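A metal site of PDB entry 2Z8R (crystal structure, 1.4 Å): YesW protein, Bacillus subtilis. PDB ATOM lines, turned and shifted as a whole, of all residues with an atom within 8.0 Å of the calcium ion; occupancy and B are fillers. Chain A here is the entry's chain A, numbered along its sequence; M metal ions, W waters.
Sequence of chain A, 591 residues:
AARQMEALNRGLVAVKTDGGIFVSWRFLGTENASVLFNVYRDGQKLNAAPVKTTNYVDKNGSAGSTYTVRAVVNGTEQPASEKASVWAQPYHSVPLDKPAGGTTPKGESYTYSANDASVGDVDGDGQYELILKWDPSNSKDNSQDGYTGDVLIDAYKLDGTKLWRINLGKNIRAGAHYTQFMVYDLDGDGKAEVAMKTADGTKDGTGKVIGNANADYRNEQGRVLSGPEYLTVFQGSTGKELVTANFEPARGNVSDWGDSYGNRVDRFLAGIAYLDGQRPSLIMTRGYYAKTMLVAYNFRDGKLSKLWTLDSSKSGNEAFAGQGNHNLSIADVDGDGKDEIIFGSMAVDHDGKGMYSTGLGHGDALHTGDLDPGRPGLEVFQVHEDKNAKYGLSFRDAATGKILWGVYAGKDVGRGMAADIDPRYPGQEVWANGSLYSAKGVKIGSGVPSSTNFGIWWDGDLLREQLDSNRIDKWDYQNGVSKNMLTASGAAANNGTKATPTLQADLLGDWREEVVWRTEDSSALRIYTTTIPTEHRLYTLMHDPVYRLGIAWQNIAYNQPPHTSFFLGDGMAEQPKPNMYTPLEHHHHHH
The calcium ion is bound by O of Asn 555 (2.3 Å). Water W1 binds the calcium ion (2.3 Å). O of Ala 557 binds the calcium ion. The calcium ion is bound by water W2, 2.4 Å away. The calcium ion is bound by OD2 of Asp 116 (2.4 Å). OD1 of Asn 559 is bound to the calcium ion, 2.4 Å away.
Water W2 lies within hydrogen-bond range of the backbone carbonyl oxygen of Ala 176 (2.8 Å), the side-chain amino group of Lys 133 (3.0 Å) and the backbone NH of Ala 557 (3.3 Å).
OD1 of Asn 555 sits close to O of Phe 181 (3.0 Å). The backbone NH (N) of Ala 557 lies close to the side-chain amide nitrogen (NE2) of Gln 180, at 2.9 Å. The backbone NH of Lys 133 sits at hydrogen-bond distance from the backbone carbonyl oxygen of Asp 116, at 2.9 Å. The side-chain carboxylate (OD1) of Asp 116 is in hydrogen-bond range of the side-chain amide nitrogen (ND2) of Asn 495 (3.1 Å). OD1 of Asp 116 sits close to OD1 of Asn 115, 3.4 Å away. O of Gln 554 sits close to ND2 of Asn 559 (3.4 Å).
Merely in contact with the calcium ion: Ile 556 (3.8 Å). Of the 24 residues printed, 5 come within 4 Å of the calcium ion.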
ATOM      1  N   ASN A 115      16.588 -24.681  22.857  1.00  0.00           N
ATOM      2  CA  ASN A 115      15.484 -24.485  21.928  1.00  0.00           C
ATOM      3  C   ASN A 115      15.196 -22.973  21.781  1.00  0.00           C
ATOM      4  O   ASN A 115      16.131 -22.173  21.686  1.00  0.00           O
ATOM      5  CB  ASN A 115      14.281 -25.346  22.389  1.00  0.00           C
ATOM      6  CG  ASN A 115      13.237 -25.543  21.311  1.00  0.00           C
ATOM      7  OD1 ASN A 115      12.227 -24.832  21.300  1.00  0.00           O
ATOM      8  ND2 ASN A 115      13.438 -26.522  20.412  1.00  0.00           N
ATOM      9  N   ASP A 116      13.926 -22.577  21.750  1.00  0.00           N
ATOM     10  CA  ASP A 116      13.568 -21.174  21.545  1.00  0.00           C
ATOM     11  C   ASP A 116      14.054 -20.296  22.675  1.00  0.00           C
ATOM     12  O   ASP A 116      14.027 -20.699  23.831  1.00  0.00           O
ATOM     13  CB  ASP A 116      12.052 -21.004  21.492  1.00  0.00           C
ATOM     14  CG  ASP A 116      11.387 -21.830  20.417  1.00  0.00           C
ATOM     15  OD1 ASP A 116      11.995 -22.080  19.348  1.00  0.00           O
ATOM     16  OD2 ASP A 116      10.222 -22.208  20.646  1.00  0.00           O
ATOM     17  N   ALA A 117      14.449 -19.078  22.322  1.00  0.00           N
ATOM     18  CA  ALA A 117      14.815 -18.086  23.305  1.00  0.00           C
ATOM     19  C   ALA A 117      14.025 -16.779  23.123  1.00  0.00           C
ATOM     20  O   ALA A 117      13.341 -16.550  22.109  1.00  0.00           O
ATOM     21  CB  ALA A 117      16.323 -17.796  23.245  1.00  0.00           C
ATOM     22  N   LYS A 133      14.548 -21.606  26.514  1.00  0.00           N
ATOM     23  CA  LYS A 133      13.749 -22.804  26.740  1.00  0.00           C
ATOM     24  C   LYS A 133      14.527 -24.043  26.311  1.00  0.00           C
ATOM     25  O   LYS A 133      15.042 -24.108  25.182  1.00  0.00           O
ATOM     26  CB  LYS A 133      12.442 -22.708  25.928  1.00  0.00           C
ATOM     27  CG  LYS A 133      11.476 -23.876  26.192  1.00  0.00           C
ATOM     28  CD  LYS A 133      10.183 -23.759  25.367  1.00  0.00           C
ATOM     29  CE  LYS A 133      10.449 -24.082  23.909  1.00  0.00           C
ATOM     30  NZ  LYS A 133       9.247 -23.790  23.038  1.00  0.00           N
ATOM     31  N   GLY A 175       6.376 -29.316  24.309  1.00  0.00           N
ATOM     32  CA  GLY A 175       6.017 -29.298  22.894  1.00  0.00           C
ATOM     33  C   GLY A 175       5.818 -27.870  22.429  1.00  0.00           C
ATOM     34  O   GLY A 175       5.608 -26.958  23.242  1.00  0.00           O
ATOM     35  N   ALA A 176       5.877 -27.665  21.107  1.00  0.00           N
ATOM     36  CA  ALA A 176       5.859 -26.336  20.524  1.00  0.00           C
ATOM     37  C   ALA A 176       4.648 -25.502  20.957  1.00  0.00           C
ATOM     38  O   ALA A 176       4.734 -24.280  21.092  1.00  0.00           O
ATOM     39  CB  ALA A 176       5.910 -26.414  19.004  1.00  0.00           C
ATOM     40  N   HIS A 177       3.503 -26.168  21.145  1.00  0.00           N
ATOM     41  CA  HIS A 177       2.246 -25.445  21.315  1.00  0.00           C
ATOM     42  C   HIS A 177       1.831 -25.266  22.754  1.00  0.00           C
ATOM     43  O   HIS A 177       0.791 -24.687  23.025  1.00  0.00           O
ATOM     44  CB  HIS A 177       1.155 -26.106  20.462  1.00  0.00           C
ATOM     45  CG  HIS A 177       1.556 -26.212  19.035  1.00  0.00           C
ATOM     46  ND1 HIS A 177       1.714 -25.103  18.227  1.00  0.00           N
ATOM     47  CD2 HIS A 177       1.969 -27.274  18.297  1.00  0.00           C
ATOM     48  CE1 HIS A 177       2.156 -25.488  17.044  1.00  0.00           C
ATOM     49  NE2 HIS A 177       2.302 -26.798  17.061  1.00  0.00           N
ATOM     50  N   THR A 179       4.099 -24.385  26.301  1.00  0.00           N
ATOM     51  CA  THR A 179       4.633 -23.171  26.932  1.00  0.00           C
ATOM     52  C   THR A 179       4.954 -22.085  25.922  1.00  0.00           C
ATOM     53  O   THR A 179       5.685 -22.318  24.960  1.00  0.00           O
ATOM     54  CB  THR A 179       5.906 -23.475  27.747  1.00  0.00           C
ATOM     55  OG1 THR A 179       5.613 -24.424  28.765  1.00  0.00           O
ATOM     56  CG2 THR A 179       6.471 -22.210  28.391  1.00  0.00           C
ATOM     57  N   GLN A 180       4.390 -20.895  26.154  1.00  0.00           N
ATOM     58  CA  GLN A 180       4.633 -19.699  25.350  1.00  0.00           C
ATOM     59  C   GLN A 180       5.069 -18.636  26.338  1.00  0.00           C
ATOM     60  O   GLN A 180       4.276 -18.194  27.174  1.00  0.00           O
ATOM     61  CB  GLN A 180       3.342 -19.249  24.636  1.00  0.00           C
ATOM     62  CG  GLN A 180       2.554 -20.410  23.968  1.00  0.00           C
ATOM     63  CD  GLN A 180       3.359 -21.268  22.981  1.00  0.00           C
ATOM     64  OE1 GLN A 180       3.020 -22.443  22.731  1.00  0.00           O
ATOM     65  NE2 GLN A 180       4.398 -20.686  22.411  1.00  0.00           N
ATOM     66  N   PHE A 181       6.347 -18.252  26.287  1.00  0.00           N
ATOM     67  CA  PHE A 181       6.895 -17.436  27.380  1.00  0.00           C
ATOM     68  C   PHE A 181       7.155 -16.002  26.970  1.00  0.00           C
ATOM     69  O   PHE A 181       7.804 -15.751  25.950  1.00  0.00           O
ATOM     70  CB  PHE A 181       8.128 -18.094  28.036  1.00  0.00           C
ATOM     71  CG  PHE A 181       9.294 -18.332  27.096  1.00  0.00           C
ATOM     72  CD1 PHE A 181      10.431 -17.505  27.136  1.00  0.00           C
ATOM     73  CD2 PHE A 181       9.280 -19.402  26.210  1.00  0.00           C
ATOM     74  CE1 PHE A 181      11.518 -17.745  26.298  1.00  0.00           C
ATOM     75  CE2 PHE A 181      10.367 -19.637  25.360  1.00  0.00           C
ATOM     76  CZ  PHE A 181      11.478 -18.799  25.404  1.00  0.00           C
ATOM     77  N   HIS A 326      -0.686 -20.938  14.014  1.00  0.00           N
ATOM     78  CA  HIS A 326       0.313 -21.288  15.041  1.00  0.00           C
ATOM     79  C   HIS A 326       1.258 -20.106  15.342  1.00  0.00           C
ATOM     80  O   HIS A 326       2.448 -20.292  15.655  1.00  0.00           O
ATOM     81  CB  HIS A 326       1.203 -22.459  14.602  1.00  0.00           C
ATOM     82  CG  HIS A 326       0.467 -23.624  14.032  1.00  0.00           C
ATOM     83  ND1 HIS A 326      -0.221 -24.527  14.811  1.00  0.00           N
ATOM     84  CD2 HIS A 326       0.378 -24.060  12.759  1.00  0.00           C
ATOM     85  CE1 HIS A 326      -0.727 -25.463  14.036  1.00  0.00           C
ATOM     86  NE2 HIS A 326      -0.370 -25.218  12.788  1.00  0.00           N
ATOM     87  N   ASN A 494      16.648 -25.397  15.243  1.00  0.00           N
ATOM     88  CA  ASN A 494      15.781 -26.130  16.167  1.00  0.00           C
ATOM     89  C   ASN A 494      14.460 -26.525  15.516  1.00  0.00           C
ATOM     90  O   ASN A 494      14.110 -26.050  14.427  1.00  0.00           O
ATOM     91  CB  ASN A 494      15.445 -25.275  17.403  1.00  0.00           C
ATOM     92  CG  ASN A 494      16.669 -24.634  18.054  1.00  0.00           C
ATOM     93  OD1 ASN A 494      16.564 -23.536  18.623  1.00  0.00           O
ATOM     94  ND2 ASN A 494      17.795 -25.307  18.007  1.00  0.00           N
ATOM     95  N   ASN A 495      13.722 -27.376  16.223  1.00  0.00           N
ATOM     96  CA  ASN A 495      12.322 -27.648  15.898  1.00  0.00           C
ATOM     97  C   ASN A 495      12.121 -28.439  14.616  1.00  0.00           C
ATOM     98  O   ASN A 495      11.161 -28.240  13.866  1.00  0.00           O
ATOM     99  CB  ASN A 495      11.492 -26.361  15.935  1.00  0.00           C
ATOM    100  CG  ASN A 495      11.488 -25.719  17.308  1.00  0.00           C
ATOM    101  OD1 ASN A 495      11.362 -26.417  18.319  1.00  0.00           O
ATOM    102  ND2 ASN A 495      11.659 -24.397  17.354  1.00  0.00           N
ATOM    103  N   LYS A 498      11.003 -27.312  10.955  1.00  0.00           N
ATOM    104  CA  LYS A 498      10.806 -25.867  11.048  1.00  0.00           C
ATOM    105  C   LYS A 498      12.149 -25.125  10.992  1.00  0.00           C
ATOM    106  O   LYS A 498      12.216 -23.996  10.515  1.00  0.00           O
ATOM    107  CB  LYS A 498      10.034 -25.487  12.315  1.00  0.00           C
ATOM    108  CG  LYS A 498       8.596 -26.028  12.364  1.00  0.00           C
ATOM    109  CD  LYS A 498       7.677 -25.318  11.369  1.00  0.00           C
ATOM    110  CE  LYS A 498       6.296 -25.968  11.325  1.00  0.00           C
ATOM    111  NZ  LYS A 498       5.384 -25.300  10.337  1.00  0.00           N
ATOM    112  N   THR A 500      14.387 -23.476  12.939  1.00  0.00           N
ATOM    113  CA  THR A 500      14.404 -22.087  13.393  1.00  0.00           C
ATOM    114  C   THR A 500      15.643 -21.829  14.255  1.00  0.00           C
ATOM    115  O   THR A 500      16.107 -22.714  14.962  1.00  0.00           O
ATOM    116  CB  THR A 500      13.146 -21.774  14.225  1.00  0.00           C
ATOM    117  OG1 THR A 500      13.016 -22.734  15.279  1.00  0.00           O
ATOM    118  CG2 THR A 500      11.897 -21.810  13.349  1.00  0.00           C
ATOM    119  N   PRO A 501      16.154 -20.593  14.228  1.00  0.00           N
ATOM    120  CA  PRO A 501      17.270 -20.291  15.127  1.00  0.00           C
ATOM    121  C   PRO A 501      16.747 -20.162  16.552  1.00  0.00           C
ATOM    122  O   PRO A 501      15.553 -19.903  16.751  1.00  0.00           O
ATOM    123  CB  PRO A 501      17.768 -18.927  14.634  1.00  0.00           C
ATOM    124  CG  PRO A 501      16.545 -18.269  14.054  1.00  0.00           C
ATOM    125  CD  PRO A 501      15.737 -19.408  13.446  1.00  0.00           C
ATOM    126  N   TRP A 553       7.271 -12.212  20.781  1.00  0.00           N
ATOM    127  CA  TRP A 553       6.518 -13.395  20.369  1.00  0.00           C
ATOM    128  C   TRP A 553       7.278 -14.370  19.466  1.00  0.00           C
ATOM    129  O   TRP A 553       6.706 -15.379  19.048  1.00  0.00           O
ATOM    130  CB  TRP A 553       5.111 -13.092  19.810  1.00  0.00           C
ATOM    131  CG  TRP A 553       5.000 -12.112  18.637  1.00  0.00           C
ATOM    132  CD1 TRP A 553       4.334 -10.909  18.660  1.00  0.00           C
ATOM    133  CD2 TRP A 553       5.477 -12.281  17.279  1.00  0.00           C
ATOM    134  NE1 TRP A 553       4.403 -10.310  17.430  1.00  0.00           N
ATOM    135  CE2 TRP A 553       5.106 -11.120  16.565  1.00  0.00           C
ATOM    136  CE3 TRP A 553       6.235 -13.265  16.614  1.00  0.00           C
ATOM    137  CZ2 TRP A 553       5.439 -10.918  15.217  1.00  0.00           C
ATOM    138  CZ3 TRP A 553       6.583 -13.047  15.266  1.00  0.00           C
ATOM    139  CH2 TRP A 553       6.175 -11.894  14.586  1.00  0.00           C
ATOM    140  N   GLN A 554       8.556 -14.101  19.167  1.00  0.00           N
ATOM    141  CA  GLN A 554       9.272 -14.986  18.236  1.00  0.00           C
ATOM    142  C   GLN A 554       9.206 -16.458  18.658  1.00  0.00           C
ATOM    143  O   GLN A 554       9.014 -17.341  17.811  1.00  0.00           O
ATOM    144  CB  GLN A 554      10.721 -14.575  18.055  1.00  0.00           C
ATOM    145  CG  GLN A 554      11.361 -15.276  16.868  1.00  0.00           C
ATOM    146  CD  GLN A 554      12.670 -14.657  16.507  1.00  0.00           C
ATOM    147  OE1 GLN A 554      12.741 -13.471  16.150  1.00  0.00           O
ATOM    148  NE2 GLN A 554      13.733 -15.438  16.605  1.00  0.00           N
ATOM    149  N   ASN A 555       9.347 -16.714  19.955  1.00  0.00           N
ATOM    150  CA  ASN A 555       9.362 -18.100  20.419  1.00  0.00           C
ATOM    151  C   ASN A 555       8.054 -18.817  20.213  1.00  0.00           C
ATOM    152  O   ASN A 555       8.035 -20.042  20.124  1.00  0.00           O
ATOM    153  CB  ASN A 555       9.780 -18.220  21.901  1.00  0.00           C
ATOM    154  CG  ASN A 555       8.735 -17.683  22.860  1.00  0.00           C
ATOM    155  OD1 ASN A 555       8.755 -16.497  23.230  1.00  0.00           O
ATOM    156  ND2 ASN A 555       7.822 -18.539  23.282  1.00  0.00           N
ATOM    157  N   ILE A 556       6.945 -18.092  20.168  1.00  0.00           N
ATOM    158  CA  ILE A 556       5.659 -18.802  20.313  1.00  0.00           C
ATOM    159  C   ILE A 556       5.361 -19.781  19.178  1.00  0.00           C
ATOM    160  O   ILE A 556       5.583 -19.496  17.996  1.00  0.00           O
ATOM    161  CB  ILE A 556       4.473 -17.874  20.593  1.00  0.00           C
ATOM    162  CG1 ILE A 556       4.007 -17.141  19.344  1.00  0.00           C
ATOM    163  CG2 ILE A 556       4.821 -16.892  21.746  1.00  0.00           C
ATOM    164  CD1 ILE A 556       2.703 -16.344  19.564  1.00  0.00           C
ATOM    165  N   ALA A 557       4.891 -20.959  19.583  1.00  0.00           N
ATOM    166  CA  ALA A 557       4.444 -21.997  18.665  1.00  0.00           C
ATOM    167  C   ALA A 557       5.390 -22.062  17.461  1.00  0.00           C
ATOM    168  O   ALA A 557       6.577 -22.306  17.653  1.00  0.00           O
ATOM    169  CB  ALA A 557       2.976 -21.768  18.280  1.00  0.00           C
ATOM    170  N   TYR A 558       4.884 -21.870  16.231  1.00  0.00           N
ATOM    171  CA  TYR A 558       5.760 -21.927  15.059  1.00  0.00           C
ATOM    172  C   TYR A 558       6.361 -20.563  14.802  1.00  0.00           C
ATOM    173  O   TYR A 558       5.760 -19.696  14.161  1.00  0.00           O
ATOM    174  CB  TYR A 558       5.045 -22.467  13.826  1.00  0.00           C
ATOM    175  CG  TYR A 558       4.626 -23.920  13.938  1.00  0.00           C
ATOM    176  CD1 TYR A 558       5.197 -24.792  14.872  1.00  0.00           C
ATOM    177  CD2 TYR A 558       3.650 -24.433  13.075  1.00  0.00           C
ATOM    178  CE1 TYR A 558       4.796 -26.132  14.944  1.00  0.00           C
ATOM    179  CE2 TYR A 558       3.256 -25.773  13.140  1.00  0.00           C
ATOM    180  CZ  TYR A 558       3.830 -26.606  14.088  1.00  0.00           C
ATOM    181  OH  TYR A 558       3.431 -27.934  14.188  1.00  0.00           O
ATOM    182  N   ASN A 559       7.566 -20.392  15.358  1.00  0.00           N
ATOM    183  CA  ASN A 559       8.321 -19.145  15.332  1.00  0.00           C
ATOM    184  C   ASN A 559       8.258 -18.467  13.970  1.00  0.00           C
ATOM    185  O   ASN A 559       8.552 -19.094  12.956  1.00  0.00           O
ATOM    186  CB  ASN A 559       9.821 -19.426  15.599  1.00  0.00           C
ATOM    187  CG  ASN A 559      10.082 -20.211  16.871  1.00  0.00           C
ATOM    188  OD1 ASN A 559       9.313 -21.105  17.274  1.00  0.00           O
ATOM    189  ND2 ASN A 559      11.242 -19.945  17.477  1.00  0.00           N
ATOM    190  N   GLN A 560       7.926 -17.178  13.964  1.00  0.00           N
ATOM    191  CA  GLN A 560       7.939 -16.367  12.744  1.00  0.00           C
ATOM    192  C   GLN A 560       8.954 -15.233  12.869  1.00  0.00           C
ATOM    193  O   GLN A 560       9.258 -14.798  13.971  1.00  0.00           O
ATOM    194  CB  GLN A 560       6.537 -15.780  12.474  1.00  0.00           C
ATOM    195  CG  GLN A 560       5.454 -16.834  12.288  1.00  0.00           C
ATOM    196  CD  GLN A 560       5.673 -17.698  11.069  1.00  0.00           C
ATOM    197  OE1 GLN A 560       5.894 -18.920  11.190  1.00  0.00           O
ATOM    198  NE2 GLN A 560       5.654 -17.077   9.921  1.00  0.00           N
HETATM  199 CA    CA M   1       8.345 -22.147  19.206  1.00  0.00          CA
HETATM  200  O   HOH W   1       8.633 -24.405  18.736  1.00  0.00           O
HETATM  201  O   HOH W   2       7.113 -22.816  21.109  1.00  0.00           O
